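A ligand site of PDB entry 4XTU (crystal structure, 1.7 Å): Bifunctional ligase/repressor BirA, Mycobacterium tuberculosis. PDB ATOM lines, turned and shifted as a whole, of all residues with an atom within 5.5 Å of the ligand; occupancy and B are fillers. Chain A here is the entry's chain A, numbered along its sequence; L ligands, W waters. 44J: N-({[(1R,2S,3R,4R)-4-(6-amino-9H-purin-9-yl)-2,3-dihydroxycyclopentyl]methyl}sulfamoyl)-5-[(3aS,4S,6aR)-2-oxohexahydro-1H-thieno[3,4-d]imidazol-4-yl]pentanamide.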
ATOM      1  N   GLY A  41      21.665   3.182  30.413  1.00  0.00           N
ATOM      2  CA  GLY A  41      21.080   1.902  30.762  1.00  0.00           C
ATOM      3  C   GLY A  41      20.923   1.024  29.534  1.00  0.00           C
ATOM      4  O   GLY A  41      21.389  -0.109  29.499  1.00  0.00           O
ATOM      5  N   SER A  42      20.285   1.568  28.504  1.00  0.00           N
ATOM      6  CA  SER A  42      20.056   0.849  27.257  1.00  0.00           C
ATOM      7  C   SER A  42      19.813   1.824  26.119  1.00  0.00           C
ATOM      8  O   SER A  42      18.886   2.632  26.174  1.00  0.00           O
ATOM      9  CB  SER A  42      18.875  -0.113  27.396  1.00  0.00           C
ATOM     10  OG  SER A  42      18.400  -0.539  26.131  1.00  0.00           O
ATOM     11  N   THR A  43      20.638   1.751  25.066  1.00  0.00           N
ATOM     12  CA  THR A  43      20.480   2.651  23.936  1.00  0.00           C
ATOM     13  C   THR A  43      19.141   2.444  23.243  1.00  0.00           C
ATOM     14  O   THR A  43      18.533   3.392  22.761  1.00  0.00           O
ATOM     15  CB  THR A  43      21.615   2.474  22.899  1.00  0.00           C
ATOM     16  OG1 THR A  43      21.671   1.110  22.473  1.00  0.00           O
ATOM     17  CG2 THR A  43      22.950   2.883  23.500  1.00  0.00           C
ATOM     18  N   ASN A  44      18.673   1.192  23.210  1.00  0.00           N
ATOM     19  CA  ASN A  44      17.363   0.898  22.647  1.00  0.00           C
ATOM     20  C   ASN A  44      16.263   1.594  23.432  1.00  0.00           C
ATOM     21  O   ASN A  44      15.380   2.239  22.853  1.00  0.00           O
ATOM     22  CB  ASN A  44      17.104  -0.611  22.614  1.00  0.00           C
ATOM     23  CG  ASN A  44      17.377  -1.216  21.252  1.00  0.00           C
ATOM     24  OD1 ASN A  44      18.218  -0.727  20.503  1.00  0.00           O
ATOM     25  ND2 ASN A  44      16.650  -2.278  20.922  1.00  0.00           N
ATOM     26  N   ALA A  45      16.313   1.481  24.758  1.00  0.00           N
ATOM     27  CA  ALA A  45      15.324   2.115  25.621  1.00  0.00           C
ATOM     28  C   ALA A  45      15.343   3.630  25.439  1.00  0.00           C
ATOM     29  O   ALA A  45      14.285   4.273  25.429  1.00  0.00           O
ATOM     30  CB  ALA A  45      15.588   1.750  27.070  1.00  0.00           C
ATOM     31  N   GLN A  67      27.217   0.370  28.659  1.00  0.00           N
ATOM     32  CA  GLN A  67      25.790   0.122  28.803  1.00  0.00           C
ATOM     33  C   GLN A  67      25.535  -0.771  30.013  1.00  0.00           C
ATOM     34  O   GLN A  67      26.013  -1.908  30.057  1.00  0.00           O
ATOM     35  CB  GLN A  67      25.230  -0.495  27.523  1.00  0.00           C
ATOM     36  CG  GLN A  67      23.722  -0.625  27.480  1.00  0.00           C
ATOM     37  CD  GLN A  67      23.221  -1.146  26.152  1.00  0.00           C
ATOM     38  OE1 GLN A  67      22.653  -0.402  25.353  1.00  0.00           O
ATOM     39  NE2 GLN A  67      23.439  -2.439  25.898  1.00  0.00           N
ATOM     40  N   ALA A  69      22.457  -1.626  31.671  1.00  0.00           N
ATOM     41  CA  ALA A  69      21.245  -2.432  31.771  1.00  0.00           C
ATOM     42  C   ALA A  69      20.762  -2.860  30.390  1.00  0.00           C
ATOM     43  O   ALA A  69      19.604  -2.642  30.032  1.00  0.00           O
ATOM     44  CB  ALA A  69      20.155  -1.665  32.505  1.00  0.00           C
ATOM     45  N   GLY A  70      21.672  -3.453  29.623  1.00  0.00           N
ATOM     46  CA  GLY A  70      21.390  -3.827  28.248  1.00  0.00           C
ATOM     47  C   GLY A  70      20.230  -4.795  28.092  1.00  0.00           C
ATOM     48  O   GLY A  70      19.982  -5.632  28.966  1.00  0.00           O
ATOM     49  N   ARG A  71      19.521  -4.662  26.977  1.00  0.00           N
ATOM     50  CA  ARG A  71      18.380  -5.516  26.678  1.00  0.00           C
ATOM     51  C   ARG A  71      18.727  -6.579  25.648  1.00  0.00           C
ATOM     52  O   ARG A  71      19.395  -6.292  24.650  1.00  0.00           O
ATOM     53  CB  ARG A  71      17.201  -4.689  26.158  1.00  0.00           C
ATOM     54  CG  ARG A  71      16.610  -3.682  27.118  1.00  0.00           C
ATOM     55  CD  ARG A  71      15.483  -2.923  26.438  1.00  0.00           C
ATOM     56  NE  ARG A  71      14.769  -2.026  27.346  1.00  0.00           N
ATOM     57  CZ  ARG A  71      13.714  -1.307  26.990  1.00  0.00           C
ATOM     58  NH1 ARG A  71      13.252  -1.375  25.744  1.00  0.00           N
ATOM     59  NH2 ARG A  71      13.121  -0.517  27.866  1.00  0.00           N
ATOM     60  N   GLY A  72      18.248  -7.799  25.881  1.00  0.00           N
ATOM     61  CA  GLY A  72      18.333  -8.850  24.888  1.00  0.00           C
ATOM     62  C   GLY A  72      16.925  -9.226  24.445  1.00  0.00           C
ATOM     63  O   GLY A  72      15.953  -8.616  24.892  1.00  0.00           O
ATOM     64  N   ARG A  73      16.813 -10.225  23.582  1.00  0.00           N
ATOM     65  CA  ARG A  73      15.503 -10.720  23.176  1.00  0.00           C
ATOM     66  C   ARG A  73      14.787 -11.423  24.330  1.00  0.00           C
ATOM     67  O   ARG A  73      15.432 -11.917  25.248  1.00  0.00           O
ATOM     68  CB  ARG A  73      15.614 -11.690  21.992  1.00  0.00           C
ATOM     69  CG  ARG A  73      16.039 -11.047  20.677  1.00  0.00           C
ATOM     70  CD  ARG A  73      16.082 -12.083  19.561  1.00  0.00           C
ATOM     71  NE  ARG A  73      16.978 -13.180  19.882  1.00  0.00           N
ATOM     72  CZ  ARG A  73      16.612 -14.460  19.932  1.00  0.00           C
ATOM     73  NH1 ARG A  73      15.357 -14.810  19.660  1.00  0.00           N
ATOM     74  NH2 ARG A  73      17.501 -15.398  20.232  1.00  0.00           N
ATOM     75  N   HIS A  74      13.461 -11.442  24.251  1.00  0.00           N
ATOM     76  CA  HIS A  74      12.622 -12.198  25.189  1.00  0.00           C
ATOM     77  C   HIS A  74      12.889 -11.861  26.649  1.00  0.00           C
ATOM     78  O   HIS A  74      12.917 -12.751  27.502  1.00  0.00           O
ATOM     79  CB  HIS A  74      12.825 -13.701  24.974  1.00  0.00           C
ATOM     80  CG  HIS A  74      12.724 -14.118  23.536  1.00  0.00           C
ATOM     81  ND1 HIS A  74      11.643 -13.795  22.741  1.00  0.00           N
ATOM     82  CD2 HIS A  74      13.566 -14.836  22.753  1.00  0.00           C
ATOM     83  CE1 HIS A  74      11.833 -14.288  21.524  1.00  0.00           C
ATOM     84  NE2 HIS A  74      12.986 -14.926  21.514  1.00  0.00           N
ATOM     85  N   ARG A  76      15.492 -11.018  28.074  1.00  0.00           N
ATOM     86  CA  ARG A  76      16.853 -11.298  28.519  1.00  0.00           C
ATOM     87  C   ARG A  76      17.682 -10.026  28.487  1.00  0.00           C
ATOM     88  O   ARG A  76      17.194  -8.963  28.095  1.00  0.00           O
ATOM     89  CB  ARG A  76      17.499 -12.390  27.655  1.00  0.00           C
ATOM     90  CG  ARG A  76      16.802 -13.740  27.764  1.00  0.00           C
ATOM     91  CD  ARG A  76      17.624 -14.849  27.108  1.00  0.00           C
ATOM     92  NE  ARG A  76      17.603 -14.768  25.655  1.00  0.00           N
ATOM     93  CZ  ARG A  76      16.859 -15.548  24.871  1.00  0.00           C
ATOM     94  NH1 ARG A  76      16.061 -16.456  25.401  1.00  0.00           N
ATOM     95  NH2 ARG A  76      16.905 -15.398  23.552  1.00  0.00           N
ATOM     96  N   GLY A  77      18.951 -10.126  28.899  1.00  0.00           N
ATOM     97  CA  GLY A  77      19.786  -8.947  28.994  1.00  0.00           C
ATOM     98  C   GLY A  77      20.924  -8.923  27.995  1.00  0.00           C
ATOM     99  O   GLY A  77      20.960  -9.702  27.035  1.00  0.00           O
ATOM    100  N   TRP A  78      21.860  -8.011  28.222  1.00  0.00           N
ATOM    101  CA  TRP A  78      23.073  -7.890  27.422  1.00  0.00           C
ATOM    102  C   TRP A  78      24.153  -7.255  28.289  1.00  0.00           C
ATOM    103  O   TRP A  78      23.945  -6.187  28.855  1.00  0.00           O
ATOM    104  CB  TRP A  78      22.825  -7.068  26.168  1.00  0.00           C
ATOM    105  CG  TRP A  78      24.007  -7.029  25.226  1.00  0.00           C
ATOM    106  CD1 TRP A  78      24.923  -6.023  25.108  1.00  0.00           C
ATOM    107  CD2 TRP A  78      24.370  -8.035  24.282  1.00  0.00           C
ATOM    108  NE1 TRP A  78      25.853  -6.354  24.147  1.00  0.00           N
ATOM    109  CE2 TRP A  78      25.539  -7.581  23.627  1.00  0.00           C
ATOM    110  CE3 TRP A  78      23.850  -9.279  23.928  1.00  0.00           C
ATOM    111  CZ2 TRP A  78      26.168  -8.328  22.624  1.00  0.00           C
ATOM    112  CZ3 TRP A  78      24.473 -10.012  22.942  1.00  0.00           C
ATOM    113  CH2 TRP A  78      25.625  -9.535  22.305  1.00  0.00           C
ATOM    114  N   ALA A  79      25.301  -7.931  28.387  1.00  0.00           N
ATOM    115  CA  ALA A  79      26.371  -7.464  29.264  1.00  0.00           C
ATOM    116  C   ALA A  79      27.436  -6.713  28.475  1.00  0.00           C
ATOM    117  O   ALA A  79      27.687  -7.003  27.302  1.00  0.00           O
ATOM    118  CB  ALA A  79      26.987  -8.634  30.001  1.00  0.00           C
ATOM    119  N   ALA A  80      28.073  -5.741  29.128  1.00  0.00           N
ATOM    120  CA  ALA A  80      29.129  -4.957  28.496  1.00  0.00           C
ATOM    121  C   ALA A  80      30.061  -4.347  29.525  1.00  0.00           C
ATOM    122  O   ALA A  80      29.684  -4.119  30.676  1.00  0.00           O
ATOM    123  CB  ALA A  80      28.522  -3.866  27.622  1.00  0.00           C
ATOM    124  N   GLN A  85      32.920  -2.660  23.353  1.00  0.00           N
ATOM    125  CA  GLN A  85      31.988  -2.977  22.278  1.00  0.00           C
ATOM    126  C   GLN A  85      31.639  -1.756  21.451  1.00  0.00           C
ATOM    127  O   GLN A  85      31.877  -0.613  21.876  1.00  0.00           O
ATOM    128  CB  GLN A  85      30.682  -3.567  22.822  1.00  0.00           C
ATOM    129  CG  GLN A  85      30.802  -4.851  23.609  1.00  0.00           C
ATOM    130  CD  GLN A  85      29.456  -5.341  24.104  1.00  0.00           C
ATOM    131  OE1 GLN A  85      28.429  -5.120  23.469  1.00  0.00           O
ATOM    132  NE2 GLN A  85      29.459  -5.996  25.259  1.00  0.00           N
ATOM    133  N   ILE A  87      28.303  -0.296  20.836  1.00  0.00           N
ATOM    134  CA  ILE A  87      26.948  -0.387  21.370  1.00  0.00           C
ATOM    135  C   ILE A  87      26.114   0.729  20.776  1.00  0.00           C
ATOM    136  O   ILE A  87      26.315   1.902  21.102  1.00  0.00           O
ATOM    137  CB  ILE A  87      26.945  -0.271  22.908  1.00  0.00           C
ATOM    138  CG1 ILE A  87      27.840  -1.339  23.531  1.00  0.00           C
ATOM    139  CG2 ILE A  87      25.527  -0.351  23.452  1.00  0.00           C
ATOM    140  CD1 ILE A  87      27.968  -1.217  25.039  1.00  0.00           C
ATOM    141  N   LEU A  88      25.191   0.397  19.880  1.00  0.00           N
ATOM    142  CA  LEU A  88      24.404   1.450  19.271  1.00  0.00           C
ATOM    143  C   LEU A  88      22.971   1.067  18.934  1.00  0.00           C
ATOM    144  O   LEU A  88      22.638  -0.113  18.804  1.00  0.00           O
ATOM    145  CB  LEU A  88      25.105   1.956  17.999  1.00  0.00           C
ATOM    146  CG  LEU A  88      25.352   1.052  16.789  1.00  0.00           C
ATOM    147  CD1 LEU A  88      24.114   0.917  15.901  1.00  0.00           C
ATOM    148  CD2 LEU A  88      26.511   1.596  15.977  1.00  0.00           C
ATOM    149  N   SER A  89      22.153   2.090  18.793  1.00  0.00           N
ATOM    150  CA  SER A  89      20.786   1.951  18.334  1.00  0.00           C
ATOM    151  C   SER A  89      20.526   2.981  17.241  1.00  0.00           C
ATOM    152  O   SER A  89      21.069   4.078  17.266  1.00  0.00           O
ATOM    153  CB  SER A  89      19.789   2.143  19.480  1.00  0.00           C
ATOM    154  OG  SER A  89      19.949   1.136  20.453  1.00  0.00           O
ATOM    155  N   ASN A 134      19.087 -13.329  14.769  1.00  0.00           N
ATOM    156  CA  ASN A 134      19.790 -12.099  15.144  1.00  0.00           C
ATOM    157  C   ASN A 134      21.243 -12.244  15.593  1.00  0.00           C
ATOM    158  O   ASN A 134      21.759 -11.366  16.282  1.00  0.00           O
ATOM    159  CB  ASN A 134      19.020 -11.409  16.260  1.00  0.00           C
ATOM    160  CG  ASN A 134      19.082 -12.183  17.571  1.00  0.00           C
ATOM    161  OD1 ASN A 134      19.054 -13.418  17.581  1.00  0.00           O
ATOM    162  ND2 ASN A 134      19.198 -11.467  18.685  1.00  0.00           N
ATOM    163  N   ASP A 135      21.919 -13.330  15.217  1.00  0.00           N
ATOM    164  CA  ASP A 135      23.246 -13.602  15.740  1.00  0.00           C
ATOM    165  C   ASP A 135      24.309 -13.507  14.661  1.00  0.00           C
ATOM    166  O   ASP A 135      24.177 -14.101  13.590  1.00  0.00           O
ATOM    167  CB  ASP A 135      23.285 -14.983  16.392  1.00  0.00           C
ATOM    168  CG  ASP A 135      22.620 -15.020  17.749  1.00  0.00           C
ATOM    169  OD1 ASP A 135      21.855 -14.082  18.060  1.00  0.00           O
ATOM    170  OD2 ASP A 135      22.840 -15.991  18.495  1.00  0.00           O
ATOM    171  N   LYS A 142      29.431 -16.028  19.793  1.00  0.00           N
ATOM    172  CA  LYS A 142      28.548 -14.914  19.463  1.00  0.00           C
ATOM    173  C   LYS A 142      29.318 -13.592  19.427  1.00  0.00           C
ATOM    174  O   LYS A 142      29.708 -13.060  20.465  1.00  0.00           O
ATOM    175  CB  LYS A 142      27.390 -14.828  20.466  1.00  0.00           C
ATOM    176  CG  LYS A 142      26.377 -13.748  20.124  1.00  0.00           C
ATOM    177  CD  LYS A 142      25.020 -14.060  20.739  1.00  0.00           C
ATOM    178  CE  LYS A 142      23.986 -13.012  20.338  1.00  0.00           C
ATOM    179  NZ  LYS A 142      22.629 -13.380  20.812  1.00  0.00           N
ATOM    180  N   ALA A 144      28.167 -10.752  17.773  1.00  0.00           N
ATOM    181  CA  ALA A 144      27.241  -9.635  17.872  1.00  0.00           C
ATOM    182  C   ALA A 144      25.803 -10.099  18.060  1.00  0.00           C
ATOM    183  O   ALA A 144      25.404 -11.152  17.559  1.00  0.00           O
ATOM    184  CB  ALA A 144      27.346  -8.731  16.644  1.00  0.00           C
ATOM    185  N   GLY A 145      25.026  -9.297  18.778  1.00  0.00           N
ATOM    186  CA  GLY A 145      23.616  -9.563  18.984  1.00  0.00           C
ATOM    187  C   GLY A 145      22.801  -8.368  18.538  1.00  0.00           C
ATOM    188  O   GLY A 145      23.213  -7.230  18.724  1.00  0.00           O
ATOM    189  N   ILE A 146      21.640  -8.635  17.950  1.00  0.00           N
ATOM    190  CA  ILE A 146      20.815  -7.557  17.422  1.00  0.00           C
ATOM    191  C   ILE A 146      19.407  -7.628  17.998  1.00  0.00           C
ATOM    192  O   ILE A 146      18.821  -8.701  18.119  1.00  0.00           O
ATOM    193  CB  ILE A 146      20.765  -7.615  15.883  1.00  0.00           C
ATOM    194  CG1 ILE A 146      22.179  -7.537  15.309  1.00  0.00           C
ATOM    195  CG2 ILE A 146      19.856  -6.514  15.330  1.00  0.00           C
ATOM    196  CD1 ILE A 146      22.307  -6.716  14.067  1.00  0.00           C
ATOM    197  N   LEU A 147      18.877  -6.466  18.380  1.00  0.00           N
ATOM    198  CA  LEU A 147      17.540  -6.396  18.952  1.00  0.00           C
ATOM    199  C   LEU A 147      16.697  -5.327  18.262  1.00  0.00           C
ATOM    200  O   LEU A 147      17.062  -4.152  18.257  1.00  0.00           O
ATOM    201  CB  LEU A 147      17.625  -6.105  20.460  1.00  0.00           C
ATOM    202  CG  LEU A 147      16.289  -6.003  21.212  1.00  0.00           C
ATOM    203  CD1 LEU A 147      15.542  -7.324  21.170  1.00  0.00           C
ATOM    204  CD2 LEU A 147      16.521  -5.550  22.647  1.00  0.00           C
ATOM    205  N   GLY A 158      18.887  -2.245  17.538  1.00  0.00           N
ATOM    206  CA  GLY A 158      20.020  -2.215  18.454  1.00  0.00           C
ATOM    207  C   GLY A 158      21.085  -3.220  18.092  1.00  0.00           C
ATOM    208  O   GLY A 158      20.793  -4.369  17.762  1.00  0.00           O
ATOM    209  N   VAL A 159      22.339  -2.786  18.149  1.00  0.00           N
ATOM    210  CA  VAL A 159      23.477  -3.653  17.842  1.00  0.00           C
ATOM    211  C   VAL A 159      24.499  -3.652  18.966  1.00  0.00           C
ATOM    212  O   VAL A 159      24.993  -2.600  19.368  1.00  0.00           O
ATOM    213  CB  VAL A 159      24.180  -3.220  16.534  1.00  0.00           C
ATOM    214  CG1 VAL A 159      25.479  -3.999  16.337  1.00  0.00           C
ATOM    215  CG2 VAL A 159      23.263  -3.399  15.342  1.00  0.00           C
ATOM    216  N   GLY A 160      24.811  -4.838  19.471  1.00  0.00           N
ATOM    217  CA  GLY A 160      25.908  -4.999  20.413  1.00  0.00           C
ATOM    218  C   GLY A 160      26.987  -5.830  19.753  1.00  0.00           C
ATOM    219  O   GLY A 160      26.799  -7.025  19.517  1.00  0.00           O
ATOM    220  N   ASN A 162      30.902  -7.173  19.893  1.00  0.00           N
ATOM    221  CA  ASN A 162      32.099  -7.358  20.709  1.00  0.00           C
ATOM    222  C   ASN A 162      33.373  -7.076  19.915  1.00  0.00           C
ATOM    223  O   ASN A 162      33.739  -7.828  19.012  1.00  0.00           O
ATOM    224  CB  ASN A 162      32.153  -8.792  21.259  1.00  0.00           C
ATOM    225  CG  ASN A 162      30.956  -9.132  22.128  1.00  0.00           C
ATOM    226  OD1 ASN A 162      30.345 -10.191  21.975  1.00  0.00           O
ATOM    227  ND2 ASN A 162      30.630  -8.245  23.047  1.00  0.00           N
ATOM    228  N   GLN A 165      35.839  -7.079  23.711  1.00  0.00           N
ATOM    229  CA  GLN A 165      35.159  -7.651  24.864  1.00  0.00           C
ATOM    230  C   GLN A 165      35.566  -9.109  25.088  1.00  0.00           C
ATOM    231  O   GLN A 165      35.393  -9.947  24.213  1.00  0.00           O
ATOM    232  CB  GLN A 165      33.646  -7.565  24.680  1.00  0.00           C
ATOM    233  CG  GLN A 165      32.847  -7.866  25.946  1.00  0.00           C
ATOM    234  CD  GLN A 165      32.786  -6.672  26.881  1.00  0.00           C
ATOM    235  OE1 GLN A 165      31.971  -5.776  26.703  1.00  0.00           O
ATOM    236  NE2 GLN A 165      33.653  -6.671  27.891  1.00  0.00           N
ATOM    237  N   VAL A 170      31.499 -11.094  29.933  1.00  0.00           N
ATOM    238  CA  VAL A 170      30.096 -10.980  29.540  1.00  0.00           C
ATOM    239  C   VAL A 170      29.325 -12.304  29.438  1.00  0.00           C
ATOM    240  O   VAL A 170      28.225 -12.410  29.969  1.00  0.00           O
ATOM    241  CB  VAL A 170      29.976 -10.238  28.181  1.00  0.00           C
ATOM    242  CG1 VAL A 170      30.251  -8.755  28.363  1.00  0.00           C
ATOM    243  CG2 VAL A 170      30.923 -10.831  27.143  1.00  0.00           C
ATOM    244  N   ASP A 171      29.896 -13.302  28.758  1.00  0.00           N
ATOM    245  CA  ASP A 171      29.189 -14.546  28.496  1.00  0.00           C
ATOM    246  C   ASP A 171      30.131 -15.607  27.932  1.00  0.00           C
ATOM    247  O   ASP A 171      30.958 -15.315  27.065  1.00  0.00           O
ATOM    248  CB  ASP A 171      28.033 -14.310  27.513  1.00  0.00           C
ATOM    249  CG  ASP A 171      27.116 -15.509  27.399  1.00  0.00           C
ATOM    250  OD1 ASP A 171      26.195 -15.634  28.240  1.00  0.00           O
ATOM    251  OD2 ASP A 171      27.302 -16.330  26.474  1.00  0.00           O
ATOM    252  N   ALA A 174      30.343 -16.143  24.130  1.00  0.00           N
ATOM    253  CA  ALA A 174      30.684 -14.958  23.358  1.00  0.00           C
ATOM    254  C   ALA A 174      32.058 -15.066  22.710  1.00  0.00           C
ATOM    255  O   ALA A 174      32.875 -15.906  23.072  1.00  0.00           O
ATOM    256  CB  ALA A 174      30.624 -13.724  24.236  1.00  0.00           C
ATOM    257  N   THR A 175      32.288 -14.198  21.724  1.00  0.00           N
ATOM    258  CA  THR A 175      33.623 -14.005  21.172  1.00  0.00           C
ATOM    259  C   THR A 175      33.753 -12.540  20.774  1.00  0.00           C
ATOM    260  O   THR A 175      32.795 -11.775  20.891  1.00  0.00           O
ATOM    261  CB  THR A 175      33.893 -14.914  19.955  1.00  0.00           C
ATOM    262  OG1 THR A 175      35.285 -14.847  19.601  1.00  0.00           O
ATOM    263  CG2 THR A 175      33.048 -14.484  18.762  1.00  0.00           C
ATOM    264  N   ASP A 265      15.029 -19.434  19.754  1.00  0.00           N
ATOM    265  CA  ASP A 265      16.473 -19.556  19.896  1.00  0.00           C
ATOM    266  C   ASP A 265      16.971 -20.781  19.146  1.00  0.00           C
ATOM    267  O   ASP A 265      16.545 -21.906  19.409  1.00  0.00           O
ATOM    268  CB  ASP A 265      16.858 -19.642  21.367  1.00  0.00           C
ATOM    269  CG  ASP A 265      16.332 -18.477  22.175  1.00  0.00           C
ATOM    270  OD1 ASP A 265      16.359 -17.338  21.671  1.00  0.00           O
ATOM    271  OD2 ASP A 265      15.875 -18.700  23.320  1.00  0.00           O
HETATM  272  CAO 44J L   1      22.671  -1.877  22.035  1.00  0.00           C
HETATM  273  CBA 44J L   1      20.240  -2.675  24.137  1.00  0.00           C
HETATM  274  CBF 44J L   1      21.163  -2.107  22.116  1.00  0.00           C
HETATM  275  CBE 44J L   1      22.046 -13.562  25.486  1.00  0.00           C
HETATM  276  CAZ 44J L   1      20.399 -10.484  21.737  1.00  0.00           C
HETATM  277  CAM 44J L   1      23.585 -13.877  27.262  1.00  0.00           C
HETATM  278  CAK 44J L   1      22.052  -5.816  22.492  1.00  0.00           C
HETATM  279  CAX 44J L   1      23.430 -13.307  24.892  1.00  0.00           C
HETATM  280  CAL 44J L   1      22.203 -13.315  26.977  1.00  0.00           C
HETATM  281  CAN 44J L   1      20.959 -12.743  24.799  1.00  0.00           C
HETATM  282  CBI 44J L   1      20.834  -3.604  22.115  1.00  0.00           C
HETATM  283  NAU 44J L   1      20.273  -3.800  23.436  1.00  0.00           N
HETATM  284  OAC 44J L   1      19.873  -2.579  25.300  1.00  0.00           O
HETATM  285  NAT 44J L   1      20.690  -1.661  23.408  1.00  0.00           N
HETATM  286  SAY 44J L   1      23.377  -3.398  22.547  1.00  0.00           S
HETATM  287  CBH 44J L   1      22.103  -4.419  21.894  1.00  0.00           C
HETATM  288  CAI 44J L   1      21.060  -6.687  21.733  1.00  0.00           C
HETATM  289  CAH 44J L   1      21.155  -8.151  22.166  1.00  0.00           C
HETATM  290  CAJ 44J L   1      20.131  -9.019  21.448  1.00  0.00           C
HETATM  291  OAB 44J L   1      21.402 -11.025  21.284  1.00  0.00           O
HETATM  292  NAV 44J L   1      19.515 -11.125  22.491  1.00  0.00           N
HETATM  293  SBK 44J L   1      19.549 -12.728  22.632  1.00  0.00           S
HETATM  294  OAD 44J L   1      18.384 -13.150  23.358  1.00  0.00           O
HETATM  295  OAE 44J L   1      19.534 -13.318  21.327  1.00  0.00           O
HETATM  296  NAW 44J L   1      20.881 -13.201  23.398  1.00  0.00           N
HETATM  297  OAL 44J L   1      22.190 -11.909  27.256  1.00  0.00           O
HETATM  298  OAM 44J L   1      24.111 -13.409  28.510  1.00  0.00           O
HETATM  299  CBG 44J L   1      24.434 -13.508  26.035  1.00  0.00           C
HETATM  300  N9  44J L   1      25.255 -12.269  26.147  1.00  0.00           N
HETATM  301  C8  44J L   1      25.173 -11.275  27.043  1.00  0.00           C
HETATM  302  N7  44J L   1      26.108 -10.334  26.762  1.00  0.00           N
HETATM  303  C5  44J L   1      26.767 -10.748  25.667  1.00  0.00           C
HETATM  304  C4  44J L   1      26.223 -11.963  25.280  1.00  0.00           C
HETATM  305  N3  44J L   1      26.710 -12.609  24.198  1.00  0.00           N
HETATM  306  C2  44J L   1      27.709 -12.078  23.492  1.00  0.00           C
HETATM  307  N1  44J L   1      28.253 -10.903  23.827  1.00  0.00           N
HETATM  308  C6  44J L   1      27.804 -10.223  24.912  1.00  0.00           C
HETATM  309  N6  44J L   1      28.362  -9.031  25.238  1.00  0.00           N
HETATM  310  O   HOH W   1      22.287 -15.793  22.493  1.00  0.00           O
HETATM  311  O   HOH W   2      26.684 -15.485  23.941  1.00  0.00           O
HETATM  312  O   HOH W   3      25.735 -11.835  31.105  1.00  0.00           O
HETATM  313  O   HOH W   4      22.999 -10.806  29.696  1.00  0.00           O
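Water W4 bridges an oxygen (OAL) of the ligand and the backbone NH (N) of Trp 78.
Water W2 bridges the side-chain carboxylate of Asp 171 and a nitrogen (N3) of the ligand.
Water W1 lies within hydrogen-bond range of the side-chain amino group of Lys 142 (3.0 Å) and a nitrogen (NAW) of the ligand (3.1 Å).
Water W3 bridges the backbone carbonyl oxygen of Val 170 (2.8 Å) and an oxygen (OAM) of the ligand (3.4 Å).
An oxygen (OAL) of the ligand sits at hydrogen-bond distance from the backbone carbonyl oxygen (O) of Gly 77 (2.5 Å).
OG of Ser 42 sits at hydrogen-bond distance from OAC of the ligand, 2.6 Å away.
An oxygen (OAB) of the ligand lies within hydrogen-bond range of the side-chain amino group (NZ) of Lys 142 (2.7 Å).
An oxygen (OAC) of the ligand lies within hydrogen-bond range of the backbone NH of Arg 71.
O of Arg 71 sits at hydrogen-bond distance from NAU of the ligand (2.9 Å).
An oxygen (OAD) of the ligand sits at hydrogen-bond distance from the guanidinium group of Arg 76 (2.7 Å).
OD1 of Asn 162 lies close to N1 of the ligand (2.9 Å).
The backbone NH of Arg 73 lies within hydrogen-bond range of a nitrogen (NAV) of the ligand, at 3.0 Å.
The guanidinium group (NE) of Arg 73 sits at hydrogen-bond distance from an oxygen (OAE) of the ligand (2.9 Å).
N of Ala 79 sits at hydrogen-bond distance from N7 of the ligand, 3.0 Å away.
A nitrogen (N6) of the ligand lies within hydrogen-bond range of the backbone carbonyl oxygen (O) of Ala 79, at 3.0 Å.
The side-chain amide oxygen (OE1) of Gln 67 is in hydrogen-bond range of a nitrogen (NAT) of the ligand.
The side-chain carboxylate of Asp 171 lies within hydrogen-bond range of an oxygen (OAM) of the ligand.
NAT of the ligand is in hydrogen-bond range of OG1 of Thr 43.
The side-chain amide nitrogen of Gln 85 sits close to a nitrogen (N6) of the ligand (3.2 Å).
ND2 of Asn 134 sits at hydrogen-bond distance from OAE of the ligand, 3.2 Å away.
SAY of the ligand sits close to N of Gly 160 (3.7 Å).
The side-chain amide nitrogen (ND2) of Asn 162 sits close to the side-chain amide nitrogen (NE2) of Gln 85, at 3.4 Å.
OD1 of Asp 265 lies within salt-bridge range of NH2 of Arg 73, 2.7 Å away.
NH1 of Arg 73 sits at hydrogen-bond distance from NE2 of His 74 (3.0 Å).
The side-chain amide oxygen of Gln 85 sits at hydrogen-bond distance from the indole nitrogen of Trp 78 (2.9 Å).
NE2 of Gln 85 is in hydrogen-bond range of OE1 of Gln 165.
O of Ile 146 sits at hydrogen-bond distance from ND2 of Asn 134 (2.8 Å).
The side-chain amide oxygen (OD1) of Asn 134 sits close to the side-chain carboxylate (OD1) of Asp 135, at 2.9 Å.
O of Gly 145 sits at hydrogen-bond distance from N of Gly 160, 3.0 Å away.
A nitrogen (NAT) of the ligand sits close to the backbone NH (N) of Asn 44 (3.5 Å).
The backbone carbonyl oxygen of Val 159 lies close to a sulfur (SAY) of the ligand (3.7 Å).
Merely in contact with the ligand: Trp 78, Ala 174, Gly 72, Gly 145, Ile 87, Gly 70, Val 170, Ile 146, Leu 88, Leu 147, Gly 158 and Ser 89.
Within 4 Å of the ligand: Ser 42, Thr 43, Asn 44, Gln 67, Gly 70, Arg 71, Gly 72, Arg 73, Arg 76, Gly 77, Trp 78, Ala 79, Gln 85, Ile 87, Leu 88, Ser 89, Asn 134, Lys 142, Gly 145, Ile 146, Leu 147, Gly 158, Val 159, Gly 160, Asn 162, Val 170, Asp 171 and Ala 174.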
